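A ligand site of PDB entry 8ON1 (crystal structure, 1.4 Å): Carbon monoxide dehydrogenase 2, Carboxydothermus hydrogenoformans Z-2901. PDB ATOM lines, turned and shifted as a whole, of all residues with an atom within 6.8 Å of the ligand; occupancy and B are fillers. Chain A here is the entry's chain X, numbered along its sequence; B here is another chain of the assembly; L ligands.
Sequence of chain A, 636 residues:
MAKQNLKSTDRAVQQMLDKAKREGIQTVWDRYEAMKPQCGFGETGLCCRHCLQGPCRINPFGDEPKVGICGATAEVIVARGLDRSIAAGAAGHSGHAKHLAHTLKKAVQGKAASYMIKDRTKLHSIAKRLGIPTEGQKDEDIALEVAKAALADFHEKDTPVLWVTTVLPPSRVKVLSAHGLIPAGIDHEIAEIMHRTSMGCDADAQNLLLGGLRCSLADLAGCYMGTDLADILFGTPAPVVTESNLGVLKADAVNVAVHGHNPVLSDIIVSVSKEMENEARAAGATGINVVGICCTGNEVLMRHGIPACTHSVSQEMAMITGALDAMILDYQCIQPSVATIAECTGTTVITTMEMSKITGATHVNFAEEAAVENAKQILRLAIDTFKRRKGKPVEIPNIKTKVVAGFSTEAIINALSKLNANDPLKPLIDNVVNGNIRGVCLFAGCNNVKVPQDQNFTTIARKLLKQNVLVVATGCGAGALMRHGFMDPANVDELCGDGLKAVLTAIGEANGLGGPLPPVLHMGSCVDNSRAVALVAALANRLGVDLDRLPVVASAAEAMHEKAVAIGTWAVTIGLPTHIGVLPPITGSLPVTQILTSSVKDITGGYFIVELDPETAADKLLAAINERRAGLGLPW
Merely in contact with the ligand: Gly 68 (3.9 Å), Ile 69 (3.8 Å) and Met 199 (3.6 Å).
Hydrophobic or aromatic side chains within 4 Å of the ligand: Ile 69 and Met 199.
Of the 27 residues printed, 11 come within 4 Å of the ligand.
The backbone carbonyl oxygen (O) of Cys 56 sits at hydrogen-bond distance from the backbone NH (N) of Cys 48 (2.8 Å).
The guanidinium group of Arg 80 lies close to the side-chain sulfur of Cys 48, 3.4 Å away.
SG of Cys 48 sits close to N of His 50, 3.4 Å away.
The side-chain sulfur (SG) of Cys 51 lies close to the backbone NH (N) of Gln 53 (3.4 Å).
N of Ala 72 lies close to SG of Cys 70 (3.6 Å).
N of Ile 69 lies close to SG of Cys 56 (3.4 Å).
O of Gln 53 sits at hydrogen-bond distance from NE2 of Gln 38 of chain B.
A ring nitrogen (ND1) of His 50 sits at hydrogen-bond distance from the backbone carbonyl oxygen (O) of Thr 197 (2.8 Å).
FE3 of the ligand is bound by SG of Cys 48, 2.3 Å away.
A sulfur (S4) of the ligand sits close to the backbone NH (N) of Cys 51.
FE2 of the ligand is bound by SG of Cys 51 (2.3 Å).
N of Cys 70 lies close to S3 of the ligand (3.5 Å).
FE4 of the ligand is bound by SG of Cys 70, at 2.3 Å.
FE1 of the ligand is bound by SG of Cys 56 (2.3 Å).
N of Gly 54 sits close to S4 of the ligand, at 3.8 Å.
S1 of the ligand lies close to NH2 of Arg 80 (3.7 Å).
The side-chain amide nitrogen (NE2) of Gln 53 sits close to a sulfur (S3) of the ligand (3.8 Å).
The backbone NH of His 50 sits close to a sulfur (S4) of the ligand (3.8 Å).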
ATOM      1  N   CYS A  47     -20.228 -22.609  13.266  1.00  0.00           N
ATOM      2  CA  CYS A  47     -21.126 -23.716  13.523  1.00  0.00           C
ATOM      3  C   CYS A  47     -22.144 -23.312  14.580  1.00  0.00           C
ATOM      4  O   CYS A  47     -21.794 -22.606  15.530  1.00  0.00           O
ATOM      5  CB  CYS A  47     -20.352 -24.910  14.079  1.00  0.00           C
ATOM      6  SG  CYS A  47     -21.463 -26.339  14.362  1.00  0.00           S
ATOM      7  N   CYS A  48     -23.397 -23.687  14.360  1.00  0.00           N
ATOM      8  CA  CYS A  48     -24.469 -23.402  15.300  1.00  0.00           C
ATOM      9  C   CYS A  48     -25.255 -24.679  15.506  1.00  0.00           C
ATOM     10  O   CYS A  48     -25.729 -25.283  14.541  1.00  0.00           O
ATOM     11  CB  CYS A  48     -25.338 -22.238  14.768  1.00  0.00           C
ATOM     12  SG  CYS A  48     -26.667 -21.860  15.899  1.00  0.00           S
ATOM     13  N   ARG A  49     -25.567 -24.983  16.750  1.00  0.00           N
ATOM     14  CA  ARG A  49     -26.463 -26.068  17.180  1.00  0.00           C
ATOM     15  C   ARG A  49     -27.552 -25.544  18.112  1.00  0.00           C
ATOM     16  O   ARG A  49     -27.984 -26.254  19.016  1.00  0.00           O
ATOM     17  CB  ARG A  49     -25.682 -27.243  17.815  1.00  0.00           C
ATOM     18  CG  ARG A  49     -24.681 -27.823  16.875  1.00  0.00           C
ATOM     19  CD  ARG A  49     -23.699 -28.737  17.562  1.00  0.00           C
ATOM     20  NE  ARG A  49     -24.416 -29.746  18.263  1.00  0.00           N
ATOM     21  CZ  ARG A  49     -24.091 -30.374  19.370  1.00  0.00           C
ATOM     22  NH1 ARG A  49     -22.910 -30.194  19.978  1.00  0.00           N
ATOM     23  NH2 ARG A  49     -24.952 -31.258  19.874  1.00  0.00           N
ATOM     24  N   HIS A  50     -27.926 -24.270  17.972  1.00  0.00           N
ATOM     25  CA  HIS A  50     -28.894 -23.679  18.920  1.00  0.00           C
ATOM     26  C   HIS A  50     -30.332 -24.103  18.683  1.00  0.00           C
ATOM     27  O   HIS A  50     -31.200 -23.716  19.458  1.00  0.00           O
ATOM     28  CB  HIS A  50     -28.757 -22.142  18.894  1.00  0.00           C
ATOM     29  CG  HIS A  50     -27.479 -21.664  19.511  1.00  0.00           C
ATOM     30  ND1 HIS A  50     -27.316 -20.380  19.938  1.00  0.00           N
ATOM     31  CD2 HIS A  50     -26.292 -22.271  19.731  1.00  0.00           C
ATOM     32  CE1 HIS A  50     -26.075 -20.209  20.404  1.00  0.00           C
ATOM     33  NE2 HIS A  50     -25.441 -21.335  20.291  1.00  0.00           N
ATOM     34  N   CYS A  51     -30.616 -24.884  17.645  1.00  0.00           N
ATOM     35  CA  CYS A  51     -31.946 -25.442  17.482  1.00  0.00           C
ATOM     36  C   CYS A  51     -31.856 -26.750  16.738  1.00  0.00           C
ATOM     37  O   CYS A  51     -30.810 -27.132  16.224  1.00  0.00           O
ATOM     38  CB  CYS A  51     -32.933 -24.486  16.856  1.00  0.00           C
ATOM     39  SG  CYS A  51     -32.884 -24.448  15.017  1.00  0.00           S
ATOM     40  N   LEU A  52     -32.953 -27.505  16.767  1.00  0.00           N
ATOM     41  CA  LEU A  52     -32.958 -28.850  16.199  1.00  0.00           C
ATOM     42  C   LEU A  52     -33.152 -28.867  14.679  1.00  0.00           C
ATOM     43  O   LEU A  52     -33.269 -29.958  14.064  1.00  0.00           O
ATOM     44  CB  LEU A  52     -34.046 -29.720  16.841  1.00  0.00           C
ATOM     45  CG  LEU A  52     -33.971 -29.783  18.366  1.00  0.00           C
ATOM     46  CD1 LEU A  52     -35.164 -30.574  18.953  1.00  0.00           C
ATOM     47  CD2 LEU A  52     -32.644 -30.463  18.715  1.00  0.00           C
ATOM     48  N   GLN A  53     -33.079 -27.705  14.036  1.00  0.00           N
ATOM     49  CA  GLN A  53     -32.932 -27.704  12.595  1.00  0.00           C
ATOM     50  C   GLN A  53     -31.482 -27.842  12.208  1.00  0.00           C
ATOM     51  O   GLN A  53     -31.195 -28.114  11.059  1.00  0.00           O
ATOM     52  CB  GLN A  53     -33.453 -26.401  11.966  1.00  0.00           C
ATOM     53  CG  GLN A  53     -34.935 -26.273  12.172  1.00  0.00           C
ATOM     54  CD  GLN A  53     -35.641 -25.036  11.597  1.00  0.00           C
ATOM     55  OE1 GLN A  53     -36.753 -25.137  11.123  1.00  0.00           O
ATOM     56  NE2 GLN A  53     -34.974 -23.878  11.604  1.00  0.00           N
ATOM     57  N   GLY A  54     -30.564 -27.558  13.145  1.00  0.00           N
ATOM     58  CA  GLY A  54     -29.140 -27.680  12.886  1.00  0.00           C
ATOM     59  C   GLY A  54     -28.679 -29.116  12.959  1.00  0.00           C
ATOM     60  O   GLY A  54     -29.502 -30.043  13.035  1.00  0.00           O
ATOM     61  N   PRO A  55     -27.400 -29.333  12.911  1.00  0.00           N
ATOM     62  CA  PRO A  55     -26.365 -28.309  12.985  1.00  0.00           C
ATOM     63  C   PRO A  55     -26.281 -27.502  11.699  1.00  0.00           C
ATOM     64  O   PRO A  55     -26.442 -28.034  10.597  1.00  0.00           O
ATOM     65  CB  PRO A  55     -25.048 -29.086  13.187  1.00  0.00           C
ATOM     66  CG  PRO A  55     -25.442 -30.435  13.386  1.00  0.00           C
ATOM     67  CD  PRO A  55     -26.839 -30.677  12.940  1.00  0.00           C
ATOM     68  N   CYS A  56     -26.001 -26.213  11.865  1.00  0.00           N
ATOM     69  CA  CYS A  56     -25.709 -25.345  10.736  1.00  0.00           C
ATOM     70  C   CYS A  56     -24.242 -24.998  10.733  1.00  0.00           C
ATOM     71  O   CYS A  56     -23.621 -24.775  11.783  1.00  0.00           O
ATOM     72  CB  CYS A  56     -26.517 -24.071  10.809  1.00  0.00           C
ATOM     73  SG  CYS A  56     -28.280 -24.355  10.533  1.00  0.00           S
ATOM     74  N   ARG A  57     -23.662 -25.024   9.575  1.00  0.00           N
ATOM     75  CA  ARG A  57     -22.283 -24.587   9.420  1.00  0.00           C
ATOM     76  C   ARG A  57     -22.250 -23.582   8.282  1.00  0.00           C
ATOM     77  O   ARG A  57     -23.185 -23.484   7.465  1.00  0.00           O
ATOM     78  CB  ARG A  57     -21.389 -25.782   9.203  1.00  0.00           C
ATOM     79  CG  ARG A  57     -21.645 -26.309   7.897  1.00  0.00           C
ATOM     80  CD  ARG A  57     -21.017 -27.689   7.630  1.00  0.00           C
ATOM     81  NE  ARG A  57     -21.264 -28.109   6.254  1.00  0.00           N
ATOM     82  CZ  ARG A  57     -22.450 -28.450   5.748  1.00  0.00           C
ATOM     83  NH1 ARG A  57     -23.584 -28.467   6.500  1.00  0.00           N
ATOM     84  NH2 ARG A  57     -22.522 -28.775   4.458  1.00  0.00           N
ATOM     85  N   VAL A  67     -25.209 -19.198   5.033  1.00  0.00           N
ATOM     86  CA  VAL A  67     -26.078 -18.636   6.054  1.00  0.00           C
ATOM     87  C   VAL A  67     -26.741 -19.795   6.753  1.00  0.00           C
ATOM     88  O   VAL A  67     -26.939 -20.860   6.162  1.00  0.00           O
ATOM     89  CB  VAL A  67     -27.075 -17.678   5.373  1.00  0.00           C
ATOM     90  CG1 VAL A  67     -27.954 -18.419   4.430  1.00  0.00           C
ATOM     91  CG2 VAL A  67     -27.835 -16.976   6.350  1.00  0.00           C
ATOM     92  N   GLY A  68     -27.046 -19.628   8.016  1.00  0.00           N
ATOM     93  CA  GLY A  68     -27.757 -20.668   8.737  1.00  0.00           C
ATOM     94  C   GLY A  68     -29.186 -20.833   8.220  1.00  0.00           C
ATOM     95  O   GLY A  68     -29.714 -19.967   7.516  1.00  0.00           O
ATOM     96  N   ILE A  69     -29.804 -21.954   8.609  1.00  0.00           N
ATOM     97  CA  ILE A  69     -31.130 -22.301   8.094  1.00  0.00           C
ATOM     98  C   ILE A  69     -32.154 -21.202   8.419  1.00  0.00           C
ATOM     99  O   ILE A  69     -32.981 -20.864   7.562  1.00  0.00           O
ATOM    100  CB  ILE A  69     -31.556 -23.719   8.577  1.00  0.00           C
ATOM    101  CG1 ILE A  69     -30.681 -24.691   7.855  1.00  0.00           C
ATOM    102  CG2 ILE A  69     -33.041 -23.977   8.299  1.00  0.00           C
ATOM    103  CD1 ILE A  69     -30.792 -26.121   8.313  1.00  0.00           C
ATOM    104  N   CYS A  70     -32.104 -20.628   9.644  1.00  0.00           N
ATOM    105  CA  CYS A  70     -33.050 -19.592  10.052  1.00  0.00           C
ATOM    106  C   CYS A  70     -32.735 -18.234   9.479  1.00  0.00           C
ATOM    107  O   CYS A  70     -33.507 -17.310   9.683  1.00  0.00           O
ATOM    108  CB  CYS A  70     -33.065 -19.507  11.515  1.00  0.00           C
ATOM    109  SG  CYS A  70     -31.443 -19.094  12.235  1.00  0.00           S
ATOM    110  N   GLY A  71     -31.621 -18.124   8.764  1.00  0.00           N
ATOM    111  CA  GLY A  71     -31.129 -16.853   8.283  1.00  0.00           C
ATOM    112  C   GLY A  71     -30.014 -16.260   9.095  1.00  0.00           C
ATOM    113  O   GLY A  71     -29.539 -15.179   8.739  1.00  0.00           O
ATOM    114  N   ALA A  72     -29.544 -16.939  10.135  1.00  0.00           N
ATOM    115  CA  ALA A  72     -28.463 -16.370  10.945  1.00  0.00           C
ATOM    116  C   ALA A  72     -27.195 -16.254  10.135  1.00  0.00           C
ATOM    117  O   ALA A  72     -26.722 -17.212   9.534  1.00  0.00           O
ATOM    118  CB  ALA A  72     -28.209 -17.252  12.141  1.00  0.00           C
ATOM    119  N   ILE A  77     -23.893 -15.902  14.204  1.00  0.00           N
ATOM    120  CA  ILE A  77     -23.486 -17.197  14.704  1.00  0.00           C
ATOM    121  C   ILE A  77     -22.231 -17.066  15.570  1.00  0.00           C
ATOM    122  O   ILE A  77     -22.188 -17.569  16.715  1.00  0.00           O
ATOM    123  CB  ILE A  77     -23.336 -18.217  13.550  1.00  0.00           C
ATOM    124  CG1 ILE A  77     -24.705 -18.611  13.006  1.00  0.00           C
ATOM    125  CG2 ILE A  77     -22.578 -19.436  14.015  1.00  0.00           C
ATOM    126  CD1 ILE A  77     -24.705 -19.440  11.788  1.00  0.00           C
ATOM    127  N   ARG A  80     -23.064 -15.096  18.864  1.00  0.00           N
ATOM    128  CA  ARG A  80     -23.863 -15.897  19.792  1.00  0.00           C
ATOM    129  C   ARG A  80     -23.006 -16.952  20.504  1.00  0.00           C
ATOM    130  O   ARG A  80     -23.153 -17.170  21.698  1.00  0.00           O
ATOM    131  CB  ARG A  80     -25.051 -16.558  19.086  1.00  0.00           C
ATOM    132  CG  ARG A  80     -26.060 -15.541  18.539  1.00  0.00           C
ATOM    133  CD  ARG A  80     -27.332 -16.188  18.144  1.00  0.00           C
ATOM    134  NE  ARG A  80     -27.160 -17.222  17.144  1.00  0.00           N
ATOM    135  CZ  ARG A  80     -28.139 -17.697  16.412  1.00  0.00           C
ATOM    136  NH1 ARG A  80     -29.390 -17.241  16.559  1.00  0.00           N
ATOM    137  NH2 ARG A  80     -27.899 -18.689  15.567  1.00  0.00           N
ATOM    138  N   THR A 197     -29.309 -15.358  22.851  1.00  0.00           N
ATOM    139  CA  THR A 197     -28.552 -16.151  21.900  1.00  0.00           C
ATOM    140  C   THR A 197     -29.335 -17.355  21.387  1.00  0.00           C
ATOM    141  O   THR A 197     -28.817 -18.074  20.521  1.00  0.00           O
ATOM    142  CB  THR A 197     -27.191 -16.567  22.484  1.00  0.00           C
ATOM    143  OG1 THR A 197     -27.424 -17.374  23.655  1.00  0.00           O
ATOM    144  CG2 THR A 197     -26.319 -15.412  22.768  1.00  0.00           C
ATOM    145  N   SER A 198     -30.484 -17.674  21.971  1.00  0.00           N
ATOM    146  CA  SER A 198     -31.292 -18.791  21.496  1.00  0.00           C
ATOM    147  C   SER A 198     -31.918 -18.414  20.126  1.00  0.00           C
ATOM    148  O   SER A 198     -31.857 -17.269  19.673  1.00  0.00           O
ATOM    149  CB  SER A 198     -32.352 -19.183  22.556  1.00  0.00           C
ATOM    150  OG  SER A 198     -33.383 -18.211  22.617  1.00  0.00           O
ATOM    151  N   MET A 199     -32.461 -19.411  19.454  1.00  0.00           N
ATOM    152  CA  MET A 199     -32.891 -19.235  18.088  1.00  0.00           C
ATOM    153  C   MET A 199     -33.981 -18.157  18.014  1.00  0.00           C
ATOM    154  O   MET A 199     -34.881 -18.039  18.842  1.00  0.00           O
ATOM    155  CB  MET A 199     -33.420 -20.533  17.544  1.00  0.00           C
ATOM    156  CG  MET A 199     -33.882 -20.562  16.097  1.00  0.00           C
ATOM    157  SD  MET A 199     -35.604 -19.928  15.981  1.00  0.00           S
ATOM    158  CE  MET A 199     -35.743 -19.692  14.267  1.00  0.00           C
ATOM    159  N   GLY A 200     -33.845 -17.316  17.014  1.00  0.00           N
ATOM    160  CA  GLY A 200     -34.905 -16.381  16.726  1.00  0.00           C
ATOM    161  C   GLY A 200     -34.949 -15.190  17.643  1.00  0.00           C
ATOM    162  O   GLY A 200     -36.013 -14.560  17.724  1.00  0.00           O
ATOM    163  N   MET B  35     -27.756 -26.550   3.194  1.00  0.00           N
ATOM    164  CA  MET B  35     -27.002 -27.040   4.339  1.00  0.00           C
ATOM    165  C   MET B  35     -26.751 -28.544   4.284  1.00  0.00           C
ATOM    166  O   MET B  35     -25.990 -29.073   5.109  1.00  0.00           O
ATOM    167  CB  MET B  35     -27.766 -26.667   5.613  1.00  0.00           C
ATOM    168  CG  MET B  35     -27.009 -26.738   6.891  1.00  0.00           C
ATOM    169  SD  MET B  35     -25.601 -25.579   6.906  1.00  0.00           S
ATOM    170  CE  MET B  35     -26.427 -24.004   7.010  1.00  0.00           C
ATOM    171  N   GLN B  38     -26.004 -32.386   6.499  1.00  0.00           N
ATOM    172  CA  GLN B  38     -25.629 -31.783   7.778  1.00  0.00           C
ATOM    173  C   GLN B  38     -24.649 -32.657   8.539  1.00  0.00           C
ATOM    174  O   GLN B  38     -24.511 -33.851   8.332  1.00  0.00           O
ATOM    175  CB  GLN B  38     -26.880 -31.534   8.622  1.00  0.00           C
ATOM    176  CG  GLN B  38     -27.725 -30.444   8.032  1.00  0.00           C
ATOM    177  CD  GLN B  38     -28.996 -30.191   8.779  1.00  0.00           C
ATOM    178  OE1 GLN B  38     -29.986 -30.940   8.679  1.00  0.00           O
ATOM    179  NE2 GLN B  38     -28.965 -29.130   9.582  1.00  0.00           N
ATOM    180  N   PRO B 336     -34.246 -14.594  11.434  1.00  0.00           N
ATOM    181  CA  PRO B 336     -33.658 -13.299  11.080  1.00  0.00           C
ATOM    182  C   PRO B 336     -33.667 -13.000   9.609  1.00  0.00           C
ATOM    183  O   PRO B 336     -33.460 -11.858   9.236  1.00  0.00           O
ATOM    184  CB  PRO B 336     -32.274 -13.351  11.725  1.00  0.00           C
ATOM    185  CG  PRO B 336     -31.972 -14.804  11.886  1.00  0.00           C
ATOM    186  CD  PRO B 336     -33.295 -15.471  12.171  1.00  0.00           C
ATOM    187  N   MET B 560     -38.316 -27.846  17.452  1.00  0.00           N
ATOM    188  CA  MET B 560     -37.164 -27.086  16.951  1.00  0.00           C
ATOM    189  C   MET B 560     -36.369 -26.354  18.047  1.00  0.00           C
ATOM    190  O   MET B 560     -35.164 -26.504  18.175  1.00  0.00           O
ATOM    191  CB  MET B 560     -37.698 -26.132  15.848  1.00  0.00           C
ATOM    192  CG  MET B 560     -36.670 -25.215  15.227  1.00  0.00           C
ATOM    193  SD  MET B 560     -36.493 -23.611  16.032  1.00  0.00           S
ATOM    194  CE  MET B 560     -37.961 -22.725  15.590  1.00  0.00           C
HETATM  195 FE1  LIG L   1     -29.275 -23.302  12.378  1.00  0.00          FE
HETATM  196 FE2  LIG L   1     -30.956 -23.324  14.382  1.00  0.00          FE
HETATM  197 FE3  LIG L   1     -28.579 -22.183  14.641  1.00  0.00          FE
HETATM  198 FE4  LIG L   1     -30.420 -20.997  13.109  1.00  0.00          FE
HETATM  199  S1  LIG L   1     -30.441 -21.338  15.355  1.00  0.00           S
HETATM  200  S2  LIG L   1     -28.313 -21.268  12.596  1.00  0.00           S
HETATM  201  S3  LIG L   1     -31.411 -22.846  12.241  1.00  0.00           S
HETATM  202  S4  LIG L   1     -29.039 -24.318  14.358  1.00  0.00           S
